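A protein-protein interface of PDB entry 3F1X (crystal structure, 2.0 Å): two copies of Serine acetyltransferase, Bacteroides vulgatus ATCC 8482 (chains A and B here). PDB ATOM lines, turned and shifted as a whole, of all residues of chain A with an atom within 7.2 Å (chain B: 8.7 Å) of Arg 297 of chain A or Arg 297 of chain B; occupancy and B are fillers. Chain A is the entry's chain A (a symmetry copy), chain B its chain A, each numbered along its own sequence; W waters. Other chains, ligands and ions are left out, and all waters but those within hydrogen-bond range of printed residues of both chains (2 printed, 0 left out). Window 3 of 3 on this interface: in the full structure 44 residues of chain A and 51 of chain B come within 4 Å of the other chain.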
ATOM      1  N   ILE A 282       9.472   4.479 -24.044  1.00  0.00           N
ATOM      2  CA  ILE A 282       8.408   5.458 -24.207  1.00  0.00           C
ATOM      3  C   ILE A 282       8.564   6.352 -25.432  1.00  0.00           C
ATOM      4  O   ILE A 282       9.672   6.708 -25.839  1.00  0.00           O
ATOM      5  CB  ILE A 282       8.255   6.348 -22.953  1.00  0.00           C
ATOM      6  CG1 ILE A 282       9.570   7.031 -22.616  1.00  0.00           C
ATOM      7  CG2 ILE A 282       7.775   5.516 -21.777  1.00  0.00           C
ATOM      8  CD1 ILE A 282       9.433   8.051 -21.500  1.00  0.00           C
ATOM      9  N   TRP A 283       7.419   6.689 -26.005  1.00  0.00           N
ATOM     10  CA  TRP A 283       7.299   7.532 -27.185  1.00  0.00           C
ATOM     11  C   TRP A 283       7.124   8.948 -26.652  1.00  0.00           C
ATOM     12  O   TRP A 283       6.053   9.303 -26.164  1.00  0.00           O
ATOM     13  CB  TRP A 283       6.070   7.047 -27.966  1.00  0.00           C
ATOM     14  CG  TRP A 283       5.674   7.812 -29.196  1.00  0.00           C
ATOM     15  CD1 TRP A 283       4.611   8.659 -29.316  1.00  0.00           C
ATOM     16  CD2 TRP A 283       6.252   7.706 -30.505  1.00  0.00           C
ATOM     17  NE1 TRP A 283       4.484   9.079 -30.618  1.00  0.00           N
ATOM     18  CE2 TRP A 283       5.481   8.514 -31.366  1.00  0.00           C
ATOM     19  CE3 TRP A 283       7.349   7.011 -31.029  1.00  0.00           C
ATOM     20  CZ2 TRP A 283       5.764   8.634 -32.729  1.00  0.00           C
ATOM     21  CZ3 TRP A 283       7.634   7.132 -32.393  1.00  0.00           C
ATOM     22  CH2 TRP A 283       6.843   7.942 -33.223  1.00  0.00           C
ATOM     23  N   VAL A 295       8.384   8.389 -17.005  1.00  0.00           N
ATOM     24  CA  VAL A 295       8.436   6.943 -17.186  1.00  0.00           C
ATOM     25  C   VAL A 295       7.151   6.374 -17.776  1.00  0.00           C
ATOM     26  O   VAL A 295       6.095   7.005 -17.723  1.00  0.00           O
ATOM     27  CB  VAL A 295       8.708   6.228 -15.844  1.00  0.00           C
ATOM     28  CG1 VAL A 295      10.071   6.632 -15.308  1.00  0.00           C
ATOM     29  CG2 VAL A 295       7.619   6.571 -14.840  1.00  0.00           C
ATOM     30  N   GLN A 296       7.255   5.170 -18.330  1.00  0.00           N
ATOM     31  CA  GLN A 296       6.115   4.497 -18.933  1.00  0.00           C
ATOM     32  C   GLN A 296       5.018   4.228 -17.902  1.00  0.00           C
ATOM     33  O   GLN A 296       5.300   3.975 -16.731  1.00  0.00           O
ATOM     34  CB  GLN A 296       6.567   3.171 -19.557  1.00  0.00           C
ATOM     35  CG  GLN A 296       5.509   2.471 -20.396  1.00  0.00           C
ATOM     36  CD  GLN A 296       5.990   1.136 -20.944  1.00  0.00           C
ATOM     37  OE1 GLN A 296       6.061   0.933 -22.161  1.00  0.00           O
ATOM     38  NE2 GLN A 296       6.326   0.221 -20.046  1.00  0.00           N
ATOM     39  N   ARG A 297       3.766   4.278 -18.351  1.00  0.00           N
ATOM     40  CA  ARG A 297       2.624   4.024 -17.481  1.00  0.00           C
ATOM     41  C   ARG A 297       2.727   2.585 -16.980  1.00  0.00           C
ATOM     42  O   ARG A 297       3.318   1.729 -17.647  1.00  0.00           O
ATOM     43  CB  ARG A 297       1.323   4.232 -18.261  1.00  0.00           C
ATOM     44  CG  ARG A 297       0.169   4.743 -17.415  1.00  0.00           C
ATOM     45  CD  ARG A 297      -1.013   5.176 -18.276  1.00  0.00           C
ATOM     46  NE  ARG A 297      -2.043   5.841 -17.480  1.00  0.00           N
ATOM     47  CZ  ARG A 297      -2.751   5.248 -16.524  1.00  0.00           C
ATOM     48  NH1 ARG A 297      -2.551   3.968 -16.240  1.00  0.00           N
ATOM     49  NH2 ARG A 297      -3.648   5.940 -15.834  1.00  0.00           N
ATOM     50  N   LYS A 298       2.156   2.317 -15.808  1.00  0.00           N
ATOM     51  CA  LYS A 298       2.205   0.983 -15.204  1.00  0.00           C
ATOM     52  C   LYS A 298       1.533  -0.098 -16.047  1.00  0.00           C
ATOM     53  O   LYS A 298       0.601   0.177 -16.805  1.00  0.00           O
ATOM     54  CB  LYS A 298       1.560   1.018 -13.817  1.00  0.00           C
ATOM     55  CG  LYS A 298       2.280   0.172 -12.776  1.00  0.00           C
ATOM     56  CD  LYS A 298       3.630   0.784 -12.418  1.00  0.00           C
ATOM     57  CE  LYS A 298       4.325   0.004 -11.311  1.00  0.00           C
ATOM     58  NZ  LYS A 298       5.600   0.654 -10.888  1.00  0.00           N
ATOM     59  N   ASN A 299       2.009  -1.333 -15.897  1.00  0.00           N
ATOM     60  CA  ASN A 299       1.478  -2.472 -16.644  1.00  0.00           C
ATOM     61  C   ASN A 299       0.772  -3.495 -15.752  1.00  0.00           C
ATOM     62  O   ASN A 299       1.192  -3.741 -14.622  1.00  0.00           O
ATOM     63  CB  ASN A 299       2.611  -3.166 -17.406  1.00  0.00           C
ATOM     64  CG  ASN A 299       3.279  -2.254 -18.418  1.00  0.00           C
ATOM     65  OD1 ASN A 299       2.641  -1.781 -19.361  1.00  0.00           O
ATOM     66  ND2 ASN A 299       4.571  -2.005 -18.229  1.00  0.00           N
ATOM     67  N   LYS A 300      -0.297  -4.091 -16.269  1.00  0.00           N
ATOM     68  CA  LYS A 300      -1.065  -5.093 -15.532  1.00  0.00           C
ATOM     69  C   LYS A 300      -2.147  -5.713 -16.413  1.00  0.00           C
ATOM     70  O   LYS A 300      -2.188  -6.956 -16.506  1.00  0.00           O
ATOM     71  CB  LYS A 300      -1.721  -4.473 -14.293  1.00  0.00           C
ATOM     72  CG  LYS A 300      -2.523  -5.466 -13.454  1.00  0.00           C
ATOM     73  CD  LYS A 300      -3.190  -4.793 -12.258  1.00  0.00           C
ATOM     74  CE  LYS A 300      -4.243  -3.781 -12.698  1.00  0.00           C
ATOM     75  NZ  LYS A 300      -4.832  -3.029 -11.550  1.00  0.00           N
ATOM     76  N   GLY B 280       5.632   4.467 -32.465  1.00  0.00           N
ATOM     77  CA  GLY B 280       6.691   3.649 -31.906  1.00  0.00           C
ATOM     78  C   GLY B 280       6.480   3.175 -30.484  1.00  0.00           C
ATOM     79  O   GLY B 280       5.576   3.636 -29.782  1.00  0.00           O
ATOM     80  N   ASN B 281       7.312   2.227 -30.073  1.00  0.00           N
ATOM     81  CA  ASN B 281       7.294   1.689 -28.714  1.00  0.00           C
ATOM     82  C   ASN B 281       6.006   1.022 -28.261  1.00  0.00           C
ATOM     83  O   ASN B 281       5.716   0.991 -27.067  1.00  0.00           O
ATOM     84  CB  ASN B 281       7.652   2.797 -27.729  1.00  0.00           C
ATOM     85  CG  ASN B 281       9.005   3.409 -28.025  1.00  0.00           C
ATOM     86  OD1 ASN B 281      10.045   2.791 -27.788  1.00  0.00           O
ATOM     87  ND2 ASN B 281       8.998   4.616 -28.567  1.00  0.00           N
ATOM     88  N   ILE B 282       5.229   0.487 -29.194  1.00  0.00           N
ATOM     89  CA  ILE B 282       3.992  -0.175 -28.810  1.00  0.00           C
ATOM     90  C   ILE B 282       3.900  -1.632 -29.252  1.00  0.00           C
ATOM     91  O   ILE B 282       4.399  -2.023 -30.309  1.00  0.00           O
ATOM     92  CB  ILE B 282       2.752   0.586 -29.333  1.00  0.00           C
ATOM     93  CG1 ILE B 282       2.826   0.760 -30.841  1.00  0.00           C
ATOM     94  CG2 ILE B 282       2.642   1.937 -28.648  1.00  0.00           C
ATOM     95  CD1 ILE B 282       1.554   1.346 -31.426  1.00  0.00           C
ATOM     96  N   ILE B 294      -2.232   4.754 -34.552  1.00  0.00           N
ATOM     97  CA  ILE B 294      -2.242   4.182 -33.212  1.00  0.00           C
ATOM     98  C   ILE B 294      -0.934   4.542 -32.517  1.00  0.00           C
ATOM     99  O   ILE B 294       0.153   4.272 -33.034  1.00  0.00           O
ATOM    100  CB  ILE B 294      -2.426   2.644 -33.262  1.00  0.00           C
ATOM    101  CG1 ILE B 294      -2.428   2.067 -31.842  1.00  0.00           C
ATOM    102  CG2 ILE B 294      -1.335   2.008 -34.095  1.00  0.00           C
ATOM    103  CD1 ILE B 294      -2.831   0.606 -31.778  1.00  0.00           C
ATOM    104  N   VAL B 295      -1.048   5.172 -31.352  1.00  0.00           N
ATOM    105  CA  VAL B 295       0.123   5.599 -30.595  1.00  0.00           C
ATOM    106  C   VAL B 295       0.082   5.152 -29.139  1.00  0.00           C
ATOM    107  O   VAL B 295      -0.980   4.827 -28.605  1.00  0.00           O
ATOM    108  CB  VAL B 295       0.268   7.137 -30.624  1.00  0.00           C
ATOM    109  CG1 VAL B 295       0.496   7.610 -32.048  1.00  0.00           C
ATOM    110  CG2 VAL B 295      -0.975   7.789 -30.038  1.00  0.00           C
ATOM    111  N   GLN B 296       1.249   5.148 -28.504  1.00  0.00           N
ATOM    112  CA  GLN B 296       1.369   4.747 -27.111  1.00  0.00           C
ATOM    113  C   GLN B 296       0.564   5.669 -26.194  1.00  0.00           C
ATOM    114  O   GLN B 296       0.439   6.866 -26.456  1.00  0.00           O
ATOM    115  CB  GLN B 296       2.843   4.767 -26.690  1.00  0.00           C
ATOM    116  CG  GLN B 296       3.120   4.172 -25.319  1.00  0.00           C
ATOM    117  CD  GLN B 296       4.588   4.268 -24.928  1.00  0.00           C
ATOM    118  OE1 GLN B 296       5.259   3.254 -24.710  1.00  0.00           O
ATOM    119  NE2 GLN B 296       5.091   5.490 -24.840  1.00  0.00           N
ATOM    120  N   ARG B 297       0.026   5.103 -25.117  1.00  0.00           N
ATOM    121  CA  ARG B 297      -0.751   5.870 -24.150  1.00  0.00           C
ATOM    122  C   ARG B 297       0.173   6.919 -23.532  1.00  0.00           C
ATOM    123  O   ARG B 297       1.392   6.726 -23.474  1.00  0.00           O
ATOM    124  CB  ARG B 297      -1.301   4.934 -23.071  1.00  0.00           C
ATOM    125  CG  ARG B 297      -2.641   5.366 -22.501  1.00  0.00           C
ATOM    126  CD  ARG B 297      -3.261   4.278 -21.630  1.00  0.00           C
ATOM    127  NE  ARG B 297      -4.628   4.618 -21.237  1.00  0.00           N
ATOM    128  CZ  ARG B 297      -4.952   5.648 -20.461  1.00  0.00           C
ATOM    129  NH1 ARG B 297      -4.008   6.446 -19.981  1.00  0.00           N
ATOM    130  NH2 ARG B 297      -6.225   5.894 -20.181  1.00  0.00           N
ATOM    131  N   LYS B 298      -0.404   8.027 -23.074  1.00  0.00           N
ATOM    132  CA  LYS B 298       0.371   9.121 -22.483  1.00  0.00           C
ATOM    133  C   LYS B 298       1.142   8.719 -21.228  1.00  0.00           C
ATOM    134  O   LYS B 298       0.733   7.817 -20.495  1.00  0.00           O
ATOM    135  CB  LYS B 298      -0.554  10.294 -22.156  1.00  0.00           C
ATOM    136  CG  LYS B 298       0.050  11.661 -22.445  1.00  0.00           C
ATOM    137  CD  LYS B 298       0.187  11.888 -23.947  1.00  0.00           C
ATOM    138  CE  LYS B 298       0.702  13.286 -24.260  1.00  0.00           C
ATOM    139  NZ  LYS B 298       0.746  13.548 -25.728  1.00  0.00           N
ATOM    140  N   ASN B 299       2.255   9.408 -20.984  1.00  0.00           N
ATOM    141  CA  ASN B 299       3.107   9.132 -19.827  1.00  0.00           C
ATOM    142  C   ASN B 299       3.128  10.278 -18.814  1.00  0.00           C
ATOM    143  O   ASN B 299       3.090  11.449 -19.187  1.00  0.00           O
ATOM    144  CB  ASN B 299       4.538   8.847 -20.294  1.00  0.00           C
ATOM    145  CG  ASN B 299       4.626   7.634 -21.200  1.00  0.00           C
ATOM    146  OD1 ASN B 299       4.303   6.515 -20.792  1.00  0.00           O
ATOM    147  ND2 ASN B 299       5.067   7.847 -22.435  1.00  0.00           N
ATOM    148  N   LYS B 300       3.195   9.931 -17.532  1.00  0.00           N
ATOM    149  CA  LYS B 300       3.228  10.921 -16.457  1.00  0.00           C
ATOM    150  C   LYS B 300       3.450  10.253 -15.102  1.00  0.00           C
ATOM    151  O   LYS B 300       4.385  10.667 -14.389  1.00  0.00           O
ATOM    152  CB  LYS B 300       1.922  11.721 -16.414  1.00  0.00           C
ATOM    153  CG  LYS B 300       1.890  12.797 -15.328  1.00  0.00           C
ATOM    154  CD  LYS B 300       0.556  13.536 -15.299  1.00  0.00           C
ATOM    155  CE  LYS B 300      -0.591  12.610 -14.904  1.00  0.00           C
ATOM    156  NZ  LYS B 300      -1.922  13.282 -14.975  1.00  0.00           N
HETATM  157  O   HOH W   1       3.821   8.590 -24.644  1.00  0.00           O
HETATM  158  O   HOH W   2       6.185   9.977 -16.079  1.00  0.00           O
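The side-chain amide nitrogen (NE2) of Gln 296 of chain B sits close to the backbone NH (N) of Trp 283 of chain A (2.9 Å). The side-chain amide oxygen (OD1) of Asn 299 of chain B sits at hydrogen-bond distance from the backbone NH (N) of Arg 297 of chain A (3.4 Å). The guanidinium group (NE) of Arg 297 of chain A sits close to the guanidinium group (NH1) of Arg 297 of chain B, at 3.2 Å.
The backbone carbonyl oxygen of Asn 281 of chain B lies close to the side-chain amide oxygen of Gln 296 of chain B. The side-chain amide nitrogen (NE2) of Gln 296 of chain B sits close to the side-chain amide nitrogen (ND2) of Asn 299 of chain B (3.4 Å). The side-chain amide nitrogen (NE2) of Gln 296 of chain A sits close to the side-chain amide nitrogen (ND2) of Asn 299 of chain A (3.4 Å).
Ile 282 of chain A touches Asn 281 of chain B (O to ND2, 3.5 Å). Ile 282 of chain A touches Gln 296 of chain B. Asn 299 of chain B touches Ile 282 of chain A. Gly 280 of chain B touches Trp 283 of chain A (N to CZ3, 3.3 Å). Trp 283 of chain A touches Asn 281 of chain B (CA to ND2, 3.6 Å). O of Val 295 of chain A touches CB of Asn 299 of chain B (3.5 Å). Gln 296 of chain A touches Gln 296 of chain B (OE1 to OE1, 3.5 Å). CA of Gln 296 of chain A touches OD1 of Asn 299 of chain B, 3.3 Å away. Arg 297 of chain A touches Lys 298 of chain B (CD to O, 3.9 Å).
Arg 297 of chain A touches three residues of chain B. Of the printed residues of chain A, Gln 296 of chain B touches Ile 282, Trp 283 and Gln 296. Printed residues of chain A within 4 Å of Asn 281 of chain B: Ile 282 and Trp 283. Lys 300 of chain A touches none of the printed residues of chain B. The nearest residue of chain B that does not touch Arg 297 of chain A is Lys 300 of chain B (5.7 Å). The nearest printed residue of chain B that does not touch Trp 283 of chain A is Asn 299 of chain B (4.1 Å).
Of the 8 printed residues of chain A, 5 touch a printed residue of chain B. Printed residues of chain A that touch a printed residue of chain B: Ile 282, Trp 283, Val 295, Gln 296 and Arg 297. Printed residues of chain B that touch a printed residue of chain A: Gly 280, Asn 281, Gln 296, Arg 297, Lys 298 and Asn 299. Among the printed residues, 12 pairs touch across the chains. Among the printed residues, no Asp or Glu carboxylate lies within 4 Å of a Lys or Arg side-chain nitrogen of the other chain.
Ile 282 of chain A touches Gln 296 of chain B, but with the chains exchanged Gln 296 of chain A does not touch Ile 282 of chain B (7.1 Å). Ile 282 of chain A touches Asn 299 of chain B, but with the chains exchanged Asn 299 of chain A does not touch Ile 282 of chain B (9.7 Å). Val 295 of chain A touches Asn 299 of chain B, but with the chains exchanged Asn 299 of chain A does not touch Val 295 of chain B (11.9 Å). Arg 297 of chain B touches its own counterpart, Arg 297 of chain A.
Water W2 bridges the backbone carbonyl oxygen (O) of Lys 300 of chain B (2.6 Å) and the backbone NH (N) of Val 295 of chain A (2.9 Å). Water W1 lies within hydrogen-bond range of ND2 of Asn 299 of chain B, O of Trp 283 of chain A, O of Arg 297 of chain B and NE2 of Gln 296 of chain B.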
